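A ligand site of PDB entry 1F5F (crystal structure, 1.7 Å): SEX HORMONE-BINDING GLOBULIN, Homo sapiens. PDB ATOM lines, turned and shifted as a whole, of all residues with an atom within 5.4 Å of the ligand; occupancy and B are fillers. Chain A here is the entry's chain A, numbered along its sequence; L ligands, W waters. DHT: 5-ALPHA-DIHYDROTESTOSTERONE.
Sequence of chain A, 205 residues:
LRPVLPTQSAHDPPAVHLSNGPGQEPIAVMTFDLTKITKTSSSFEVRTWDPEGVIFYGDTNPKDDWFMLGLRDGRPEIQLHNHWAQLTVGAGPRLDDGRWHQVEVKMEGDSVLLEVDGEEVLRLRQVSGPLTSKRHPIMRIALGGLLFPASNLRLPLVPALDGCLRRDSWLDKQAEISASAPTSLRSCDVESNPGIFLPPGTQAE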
ATOM      1  N   THR A  40     -12.974   4.576   1.743  1.00  0.00           N
ATOM      2  CA  THR A  40     -13.263   5.822   2.473  1.00  0.00           C
ATOM      3  C   THR A  40     -12.606   6.993   1.757  1.00  0.00           C
ATOM      4  O   THR A  40     -11.791   7.735   2.304  1.00  0.00           O
ATOM      5  CB  THR A  40     -12.773   5.763   3.926  1.00  0.00           C
ATOM      6  OG1 THR A  40     -11.357   5.494   3.987  1.00  0.00           O
ATOM      7  CG2 THR A  40     -13.556   4.699   4.682  1.00  0.00           C
ATOM      8  N   SER A  41     -12.994   7.119   0.496  1.00  0.00           N
ATOM      9  CA  SER A  41     -12.508   8.181  -0.337  1.00  0.00           C
ATOM     10  C   SER A  41     -13.580   8.591  -1.333  1.00  0.00           C
ATOM     11  O   SER A  41     -14.502   7.849  -1.708  1.00  0.00           O
ATOM     12  CB  SER A  41     -11.227   7.801  -1.094  1.00  0.00           C
ATOM     13  OG  SER A  41     -11.558   6.709  -1.944  1.00  0.00           O
ATOM     14  N   SER A  42     -13.461   9.809  -1.804  1.00  0.00           N
ATOM     15  CA  SER A  42     -14.322  10.410  -2.821  1.00  0.00           C
ATOM     16  C   SER A  42     -13.478  11.184  -3.824  1.00  0.00           C
ATOM     17  O   SER A  42     -12.445  11.746  -3.470  1.00  0.00           O
ATOM     18  CB  SER A  42     -15.557  11.137  -2.375  1.00  0.00           C
ATOM     19  OG  SER A  42     -16.392  10.657  -1.382  1.00  0.00           O
ATOM     20  N   PHE A  56     -19.318  19.845  -1.603  1.00  0.00           N
ATOM     21  CA  PHE A  56     -20.136  18.730  -1.039  1.00  0.00           C
ATOM     22  C   PHE A  56     -20.062  18.792   0.470  1.00  0.00           C
ATOM     23  O   PHE A  56     -19.189  19.444   1.091  1.00  0.00           O
ATOM     24  CB  PHE A  56     -19.737  17.360  -1.550  1.00  0.00           C
ATOM     25  CG  PHE A  56     -18.503  16.746  -0.922  1.00  0.00           C
ATOM     26  CD1 PHE A  56     -18.521  15.976   0.239  1.00  0.00           C
ATOM     27  CD2 PHE A  56     -17.324  16.886  -1.627  1.00  0.00           C
ATOM     28  CE1 PHE A  56     -17.360  15.406   0.714  1.00  0.00           C
ATOM     29  CE2 PHE A  56     -16.111  16.351  -1.146  1.00  0.00           C
ATOM     30  CZ  PHE A  56     -16.188  15.585   0.020  1.00  0.00           C
ATOM     31  N   GLY A  58     -20.913  16.332   4.095  1.00  0.00           N
ATOM     32  CA  GLY A  58     -21.118  14.926   4.559  1.00  0.00           C
ATOM     33  C   GLY A  58     -21.364  14.960   6.042  1.00  0.00           C
ATOM     34  O   GLY A  58     -20.859  15.802   6.795  1.00  0.00           O
ATOM     35  N   ASP A  59     -22.215  13.998   6.518  1.00  0.00           N
ATOM     36  CA  ASP A  59     -22.498  13.944   7.928  1.00  0.00           C
ATOM     37  C   ASP A  59     -22.811  12.481   8.345  1.00  0.00           C
ATOM     38  O   ASP A  59     -23.012  11.601   7.503  1.00  0.00           O
ATOM     39  CB  ASP A  59     -23.518  14.871   8.524  1.00  0.00           C
ATOM     40  CG  ASP A  59     -24.986  14.697   8.077  1.00  0.00           C
ATOM     41  OD1 ASP A  59     -25.234  13.545   7.653  1.00  0.00           O
ATOM     42  OD2 ASP A  59     -25.749  15.707   8.214  1.00  0.00           O
ATOM     43  N   THR A  60     -22.654  12.321   9.647  1.00  0.00           N
ATOM     44  CA  THR A  60     -22.997  11.015  10.244  1.00  0.00           C
ATOM     45  C   THR A  60     -24.047  11.439  11.274  1.00  0.00           C
ATOM     46  O   THR A  60     -24.786  10.634  11.821  1.00  0.00           O
ATOM     47  CB  THR A  60     -21.906  10.176  10.890  1.00  0.00           C
ATOM     48  OG1 THR A  60     -21.039  10.859  11.813  1.00  0.00           O
ATOM     49  CG2 THR A  60     -20.968   9.603   9.834  1.00  0.00           C
ATOM     50  N   ASP A  65     -21.619  15.485  13.861  1.00  0.00           N
ATOM     51  CA  ASP A  65     -20.443  14.960  13.173  1.00  0.00           C
ATOM     52  C   ASP A  65     -20.648  15.258  11.684  1.00  0.00           C
ATOM     53  O   ASP A  65     -21.389  14.584  10.957  1.00  0.00           O
ATOM     54  CB  ASP A  65     -20.350  13.426  13.233  1.00  0.00           C
ATOM     55  CG  ASP A  65     -20.353  12.755  14.602  1.00  0.00           C
ATOM     56  OD1 ASP A  65     -21.440  12.820  15.207  1.00  0.00           O
ATOM     57  OD2 ASP A  65     -19.285  12.273  14.984  1.00  0.00           O
ATOM     58  N   TRP A  66     -20.026  16.368  11.246  1.00  0.00           N
ATOM     59  CA  TRP A  66     -20.212  16.841   9.875  1.00  0.00           C
ATOM     60  C   TRP A  66     -18.944  17.357   9.243  1.00  0.00           C
ATOM     61  O   TRP A  66     -17.932  17.605   9.922  1.00  0.00           O
ATOM     62  CB  TRP A  66     -21.425  17.801   9.843  1.00  0.00           C
ATOM     63  CG  TRP A  66     -21.237  19.089  10.576  1.00  0.00           C
ATOM     64  CD1 TRP A  66     -21.601  19.326  11.867  1.00  0.00           C
ATOM     65  CD2 TRP A  66     -20.536  20.267  10.129  1.00  0.00           C
ATOM     66  NE1 TRP A  66     -21.230  20.612  12.254  1.00  0.00           N
ATOM     67  CE2 TRP A  66     -20.597  21.180  11.182  1.00  0.00           C
ATOM     68  CE3 TRP A  66     -19.904  20.591   8.930  1.00  0.00           C
ATOM     69  CZ2 TRP A  66     -19.980  22.458  11.096  1.00  0.00           C
ATOM     70  CZ3 TRP A  66     -19.318  21.868   8.817  1.00  0.00           C
ATOM     71  CH2 TRP A  66     -19.381  22.749   9.899  1.00  0.00           C
ATOM     72  N   PHE A  67     -18.942  17.441   7.922  1.00  0.00           N
ATOM     73  CA  PHE A  67     -17.860  17.873   7.088  1.00  0.00           C
ATOM     74  C   PHE A  67     -18.355  18.698   5.917  1.00  0.00           C
ATOM     75  O   PHE A  67     -19.391  18.373   5.295  1.00  0.00           O
ATOM     76  CB  PHE A  67     -17.114  16.645   6.561  1.00  0.00           C
ATOM     77  CG  PHE A  67     -16.013  16.807   5.563  1.00  0.00           C
ATOM     78  CD1 PHE A  67     -14.691  16.953   6.081  1.00  0.00           C
ATOM     79  CD2 PHE A  67     -16.228  16.966   4.199  1.00  0.00           C
ATOM     80  CE1 PHE A  67     -13.621  16.964   5.208  1.00  0.00           C
ATOM     81  CE2 PHE A  67     -15.148  17.058   3.317  1.00  0.00           C
ATOM     82  CZ  PHE A  67     -13.855  17.131   3.836  1.00  0.00           C
ATOM     83  N   LEU A  80     -14.966  21.175   9.544  1.00  0.00           N
ATOM     84  CA  LEU A  80     -15.161  19.758  10.034  1.00  0.00           C
ATOM     85  C   LEU A  80     -15.587  19.951  11.457  1.00  0.00           C
ATOM     86  O   LEU A  80     -15.046  20.797  12.205  1.00  0.00           O
ATOM     87  CB  LEU A  80     -13.726  19.129   9.920  1.00  0.00           C
ATOM     88  CG  LEU A  80     -13.514  17.675  10.293  1.00  0.00           C
ATOM     89  CD1 LEU A  80     -12.387  17.096   9.440  1.00  0.00           C
ATOM     90  CD2 LEU A  80     -13.280  17.660  11.805  1.00  0.00           C
ATOM     91  N   HIS A  81     -16.561  19.207  11.974  1.00  0.00           N
ATOM     92  CA  HIS A  81     -16.941  19.186  13.352  1.00  0.00           C
ATOM     93  C   HIS A  81     -17.303  17.769  13.772  1.00  0.00           C
ATOM     94  O   HIS A  81     -18.285  17.243  13.223  1.00  0.00           O
ATOM     95  CB  HIS A  81     -18.062  20.218  13.574  1.00  0.00           C
ATOM     96  CG  HIS A  81     -18.581  20.194  14.961  1.00  0.00           C
ATOM     97  ND1 HIS A  81     -18.399  21.295  15.773  1.00  0.00           N
ATOM     98  CD2 HIS A  81     -19.337  19.336  15.685  1.00  0.00           C
ATOM     99  CE1 HIS A  81     -18.986  21.109  16.931  1.00  0.00           C
ATOM    100  NE2 HIS A  81     -19.529  19.904  16.927  1.00  0.00           N
ATOM    101  N   ASN A  82     -16.596  17.177  14.737  1.00  0.00           N
ATOM    102  CA  ASN A  82     -16.918  15.822  15.183  1.00  0.00           C
ATOM    103  C   ASN A  82     -16.379  15.719  16.611  1.00  0.00           C
ATOM    104  O   ASN A  82     -15.991  16.711  17.221  1.00  0.00           O
ATOM    105  CB  ASN A  82     -16.426  14.763  14.180  1.00  0.00           C
ATOM    106  CG  ASN A  82     -14.922  14.656  14.022  1.00  0.00           C
ATOM    107  OD1 ASN A  82     -14.211  15.074  14.930  1.00  0.00           O
ATOM    108  ND2 ASN A  82     -14.406  14.035  12.966  1.00  0.00           N
ATOM    109  N   TRP A  84     -13.696  14.520  17.718  1.00  0.00           N
ATOM    110  CA  TRP A  84     -12.242  14.632  17.839  1.00  0.00           C
ATOM    111  C   TRP A  84     -11.767  16.037  17.462  1.00  0.00           C
ATOM    112  O   TRP A  84     -10.677  16.406  17.946  1.00  0.00           O
ATOM    113  CB  TRP A  84     -11.478  13.651  16.955  1.00  0.00           C
ATOM    114  CG  TRP A  84     -11.818  12.247  17.353  1.00  0.00           C
ATOM    115  CD1 TRP A  84     -11.297  11.523  18.392  1.00  0.00           C
ATOM    116  CD2 TRP A  84     -12.962  11.510  16.882  1.00  0.00           C
ATOM    117  NE1 TRP A  84     -11.982  10.346  18.535  1.00  0.00           N
ATOM    118  CE2 TRP A  84     -13.029  10.329  17.650  1.00  0.00           C
ATOM    119  CE3 TRP A  84     -13.964  11.793  15.940  1.00  0.00           C
ATOM    120  CZ2 TRP A  84     -14.015   9.359  17.432  1.00  0.00           C
ATOM    121  CZ3 TRP A  84     -14.898  10.789  15.688  1.00  0.00           C
ATOM    122  CH2 TRP A  84     -14.954   9.628  16.475  1.00  0.00           C
ATOM    123  N   VAL A 105     -10.812  13.459  -1.848  1.00  0.00           N
ATOM    124  CA  VAL A 105     -10.828  13.637  -0.393  1.00  0.00           C
ATOM    125  C   VAL A 105     -10.785  12.226   0.181  1.00  0.00           C
ATOM    126  O   VAL A 105     -11.625  11.410  -0.195  1.00  0.00           O
ATOM    127  CB  VAL A 105     -12.071  14.338   0.114  1.00  0.00           C
ATOM    128  CG1 VAL A 105     -11.986  14.541   1.631  1.00  0.00           C
ATOM    129  CG2 VAL A 105     -12.101  15.762  -0.486  1.00  0.00           C
ATOM    130  N   LYS A 106      -9.753  11.956   0.971  1.00  0.00           N
ATOM    131  CA  LYS A 106      -9.574  10.573   1.447  1.00  0.00           C
ATOM    132  C   LYS A 106      -9.423  10.532   2.948  1.00  0.00           C
ATOM    133  O   LYS A 106      -8.702  11.375   3.515  1.00  0.00           O
ATOM    134  CB  LYS A 106      -8.259  10.014   0.867  1.00  0.00           C
ATOM    135  CG  LYS A 106      -7.945  10.324  -0.568  1.00  0.00           C
ATOM    136  CD  LYS A 106      -6.662   9.570  -0.971  1.00  0.00           C
ATOM    137  CE  LYS A 106      -6.893   8.848  -2.292  1.00  0.00           C
ATOM    138  NZ  LYS A 106      -7.801   7.664  -2.193  1.00  0.00           N
ATOM    139  N   MET A 107      -9.934   9.490   3.582  1.00  0.00           N
ATOM    140  CA  MET A 107      -9.514   9.256   4.993  1.00  0.00           C
ATOM    141  C   MET A 107      -8.395   8.248   5.019  1.00  0.00           C
ATOM    142  O   MET A 107      -8.469   7.252   4.293  1.00  0.00           O
ATOM    143  CB  MET A 107     -10.813   8.845   5.677  1.00  0.00           C
ATOM    144  CG  MET A 107     -11.282   9.853   6.730  1.00  0.00           C
ATOM    145  SD  MET A 107     -12.019   8.895   8.101  1.00  0.00           S
ATOM    146  CE  MET A 107     -12.840   7.702   7.034  1.00  0.00           C
ATOM    147  N   VAL A 112      -7.622  13.267   7.381  1.00  0.00           N
ATOM    148  CA  VAL A 112      -8.334  13.513   6.152  1.00  0.00           C
ATOM    149  C   VAL A 112      -7.443  14.259   5.170  1.00  0.00           C
ATOM    150  O   VAL A 112      -6.837  15.276   5.542  1.00  0.00           O
ATOM    151  CB  VAL A 112      -9.637  14.284   6.435  1.00  0.00           C
ATOM    152  CG1 VAL A 112     -10.217  14.702   5.055  1.00  0.00           C
ATOM    153  CG2 VAL A 112     -10.697  13.507   7.197  1.00  0.00           C
ATOM    154  N   VAL A 127      -8.063  13.756  13.146  1.00  0.00           N
ATOM    155  CA  VAL A 127      -9.414  14.293  13.080  1.00  0.00           C
ATOM    156  C   VAL A 127     -10.474  13.195  13.046  1.00  0.00           C
ATOM    157  O   VAL A 127     -11.625  13.515  13.188  1.00  0.00           O
ATOM    158  CB  VAL A 127      -9.703  15.230  11.864  1.00  0.00           C
ATOM    159  CG1 VAL A 127      -8.768  16.420  12.025  1.00  0.00           C
ATOM    160  CG2 VAL A 127      -9.498  14.600  10.509  1.00  0.00           C
ATOM    161  N   SER A 128     -10.045  11.965  12.889  1.00  0.00           N
ATOM    162  CA  SER A 128     -11.176  11.007  12.757  1.00  0.00           C
ATOM    163  C   SER A 128     -10.952   9.785  13.620  1.00  0.00           C
ATOM    164  O   SER A 128      -9.855   9.262  13.430  1.00  0.00           O
ATOM    165  CB  SER A 128     -11.257  10.612  11.277  1.00  0.00           C
ATOM    166  OG  SER A 128     -12.441   9.791  11.123  1.00  0.00           O
ATOM    167  N   LEU A 131     -13.958   4.678  11.396  1.00  0.00           N
ATOM    168  CA  LEU A 131     -15.118   4.871  10.535  1.00  0.00           C
ATOM    169  C   LEU A 131     -16.200   3.822  10.788  1.00  0.00           C
ATOM    170  O   LEU A 131     -16.951   3.460   9.888  1.00  0.00           O
ATOM    171  CB  LEU A 131     -14.804   4.934   9.040  1.00  0.00           C
ATOM    172  CG  LEU A 131     -15.487   6.069   8.257  1.00  0.00           C
ATOM    173  CD1 LEU A 131     -15.758   5.643   6.825  1.00  0.00           C
ATOM    174  CD2 LEU A 131     -16.776   6.536   8.906  1.00  0.00           C
ATOM    175  N   MET A 139     -23.979   7.388   6.901  1.00  0.00           N
ATOM    176  CA  MET A 139     -23.302   8.644   6.450  1.00  0.00           C
ATOM    177  C   MET A 139     -24.103   9.279   5.309  1.00  0.00           C
ATOM    178  O   MET A 139     -24.606   8.546   4.424  1.00  0.00           O
ATOM    179  CB  MET A 139     -21.899   8.296   5.981  1.00  0.00           C
ATOM    180  CG  MET A 139     -21.167   9.534   5.421  1.00  0.00           C
ATOM    181  SD  MET A 139     -19.383   9.217   5.333  1.00  0.00           S
ATOM    182  CE  MET A 139     -18.913   9.139   7.054  1.00  0.00           C
ATOM    183  N   ILE A 141     -24.038  12.056   2.082  1.00  0.00           N
ATOM    184  CA  ILE A 141     -23.246  12.964   1.259  1.00  0.00           C
ATOM    185  C   ILE A 141     -24.158  13.852   0.404  1.00  0.00           C
ATOM    186  O   ILE A 141     -25.096  13.369  -0.287  1.00  0.00           O
ATOM    187  CB  ILE A 141     -22.274  12.213   0.356  1.00  0.00           C
ATOM    188  CG1 ILE A 141     -21.208  11.368   1.056  1.00  0.00           C
ATOM    189  CG2 ILE A 141     -21.600  13.229  -0.602  1.00  0.00           C
ATOM    190  CD1 ILE A 141     -20.331  12.182   1.987  1.00  0.00           C
ATOM    191  N   LEU A 171     -17.514   7.684  -1.927  1.00  0.00           N
ATOM    192  CA  LEU A 171     -17.298   6.557  -0.991  1.00  0.00           C
ATOM    193  C   LEU A 171     -17.364   5.217  -1.693  1.00  0.00           C
ATOM    194  O   LEU A 171     -16.812   4.932  -2.751  1.00  0.00           O
ATOM    195  CB  LEU A 171     -18.254   6.687   0.199  1.00  0.00           C
ATOM    196  CG  LEU A 171     -18.143   7.884   1.143  1.00  0.00           C
ATOM    197  CD1 LEU A 171     -19.379   8.020   2.018  1.00  0.00           C
ATOM    198  CD2 LEU A 171     -16.902   7.788   2.032  1.00  0.00           C
HETATM  199  C1  DHT L   1     -14.082  10.962   4.336  1.00  0.00           C
HETATM  200  C2  DHT L   1     -13.632  10.854   2.878  1.00  0.00           C
HETATM  201  C3  DHT L   1     -14.804  11.080   1.948  1.00  0.00           C
HETATM  202  O3  DHT L   1     -14.882  10.466   0.893  1.00  0.00           O
HETATM  203  C4  DHT L   1     -15.890  12.027   2.290  1.00  0.00           C
HETATM  204  C5  DHT L   1     -16.284  12.059   3.756  1.00  0.00           C
HETATM  205  C6  DHT L   1     -17.248  13.157   4.129  1.00  0.00           C
HETATM  206  C7  DHT L   1     -17.887  12.971   5.507  1.00  0.00           C
HETATM  207  C8  DHT L   1     -16.730  12.917   6.561  1.00  0.00           C
HETATM  208  C9  DHT L   1     -15.683  11.892   6.125  1.00  0.00           C
HETATM  209  C10 DHT L   1     -15.045  12.098   4.725  1.00  0.00           C
HETATM  210  C11 DHT L   1     -14.582  11.711   7.193  1.00  0.00           C
HETATM  211  C12 DHT L   1     -15.097  11.544   8.612  1.00  0.00           C
HETATM  212  C13 DHT L   1     -16.151  12.541   9.019  1.00  0.00           C
HETATM  213  C14 DHT L   1     -17.253  12.581   7.947  1.00  0.00           C
HETATM  214  C15 DHT L   1     -18.293  13.534   8.580  1.00  0.00           C
HETATM  215  C16 DHT L   1     -18.255  13.150  10.079  1.00  0.00           C
HETATM  216  C17 DHT L   1     -17.012  12.266  10.224  1.00  0.00           C
HETATM  217  O17 DHT L   1     -16.341  12.478  11.482  1.00  0.00           O
HETATM  218  C18 DHT L   1     -15.458  13.928   9.217  1.00  0.00           C
HETATM  219  C19 DHT L   1     -14.303  13.433   4.561  1.00  0.00           C
HETATM  220  O   HOH W   1     -14.900  10.298  12.031  1.00  0.00           O
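Water W1 lies within hydrogen-bond range of OG of Ser 128 (2.7 Å) and O17 of the ligand (2.7 Å).
N of Leu 171 lies within hydrogen-bond range of OG of Ser 42 (3.2 Å).
OD1 of Asn 82 lies within hydrogen-bond range of N of Trp 84.
N of Leu 171 lies within hydrogen-bond range of O of Ser 41.
O of Asp 65 sits at hydrogen-bond distance from N of Thr 60, at 2.9 Å.
The backbone carbonyl oxygen of Gly 58 sits at hydrogen-bond distance from the backbone NH of Phe 67 (2.8 Å).
The backbone carbonyl oxygen (O) of Thr 40 is in hydrogen-bond range of the backbone NH (N) of Met 107, 2.9 Å away.
The side-chain hydroxyl of Ser 128 lies within hydrogen-bond range of the side-chain sulfur of Met 107 (3.2 Å).
N of Trp 66 sits at hydrogen-bond distance from O of His 81 (2.8 Å).
Thr 40 touches the ligand.
Ser 41 touches the ligand.
Gly 58 touches the ligand.
O of Asp 65 touches C16 of the ligand (3.6 Å).
Trp 66 touches the ligand (N to C16, 3.9 Å).
Phe 67 touches the ligand.
O of Val 105 touches O3 of the ligand (3.6 Å).
Met 107 touches the ligand.
CE of Met 139 touches C14 of the ligand, 3.9 Å away.
Ile 141 touches the ligand.
CD2 of Leu 171 touches O3 of the ligand (3.5 Å).
Hydrophobic or aromatic side chains within 4 Å of the ligand: Phe 67, Val 105, Met 107, Met 139, Ile 141 and Leu 171.
The nearest printed residue that does not touch the ligand is Thr 60 (4.001 Å).
An oxygen (O3) of the ligand is in hydrogen-bond range of the backbone NH of Ser 42.
The side-chain hydroxyl (OG) of Ser 42 sits at hydrogen-bond distance from an oxygen (O3) of the ligand (2.7 Å).
The side-chain amide nitrogen of Asn 82 is in hydrogen-bond range of an oxygen (O17) of the ligand, at 2.9 Å.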
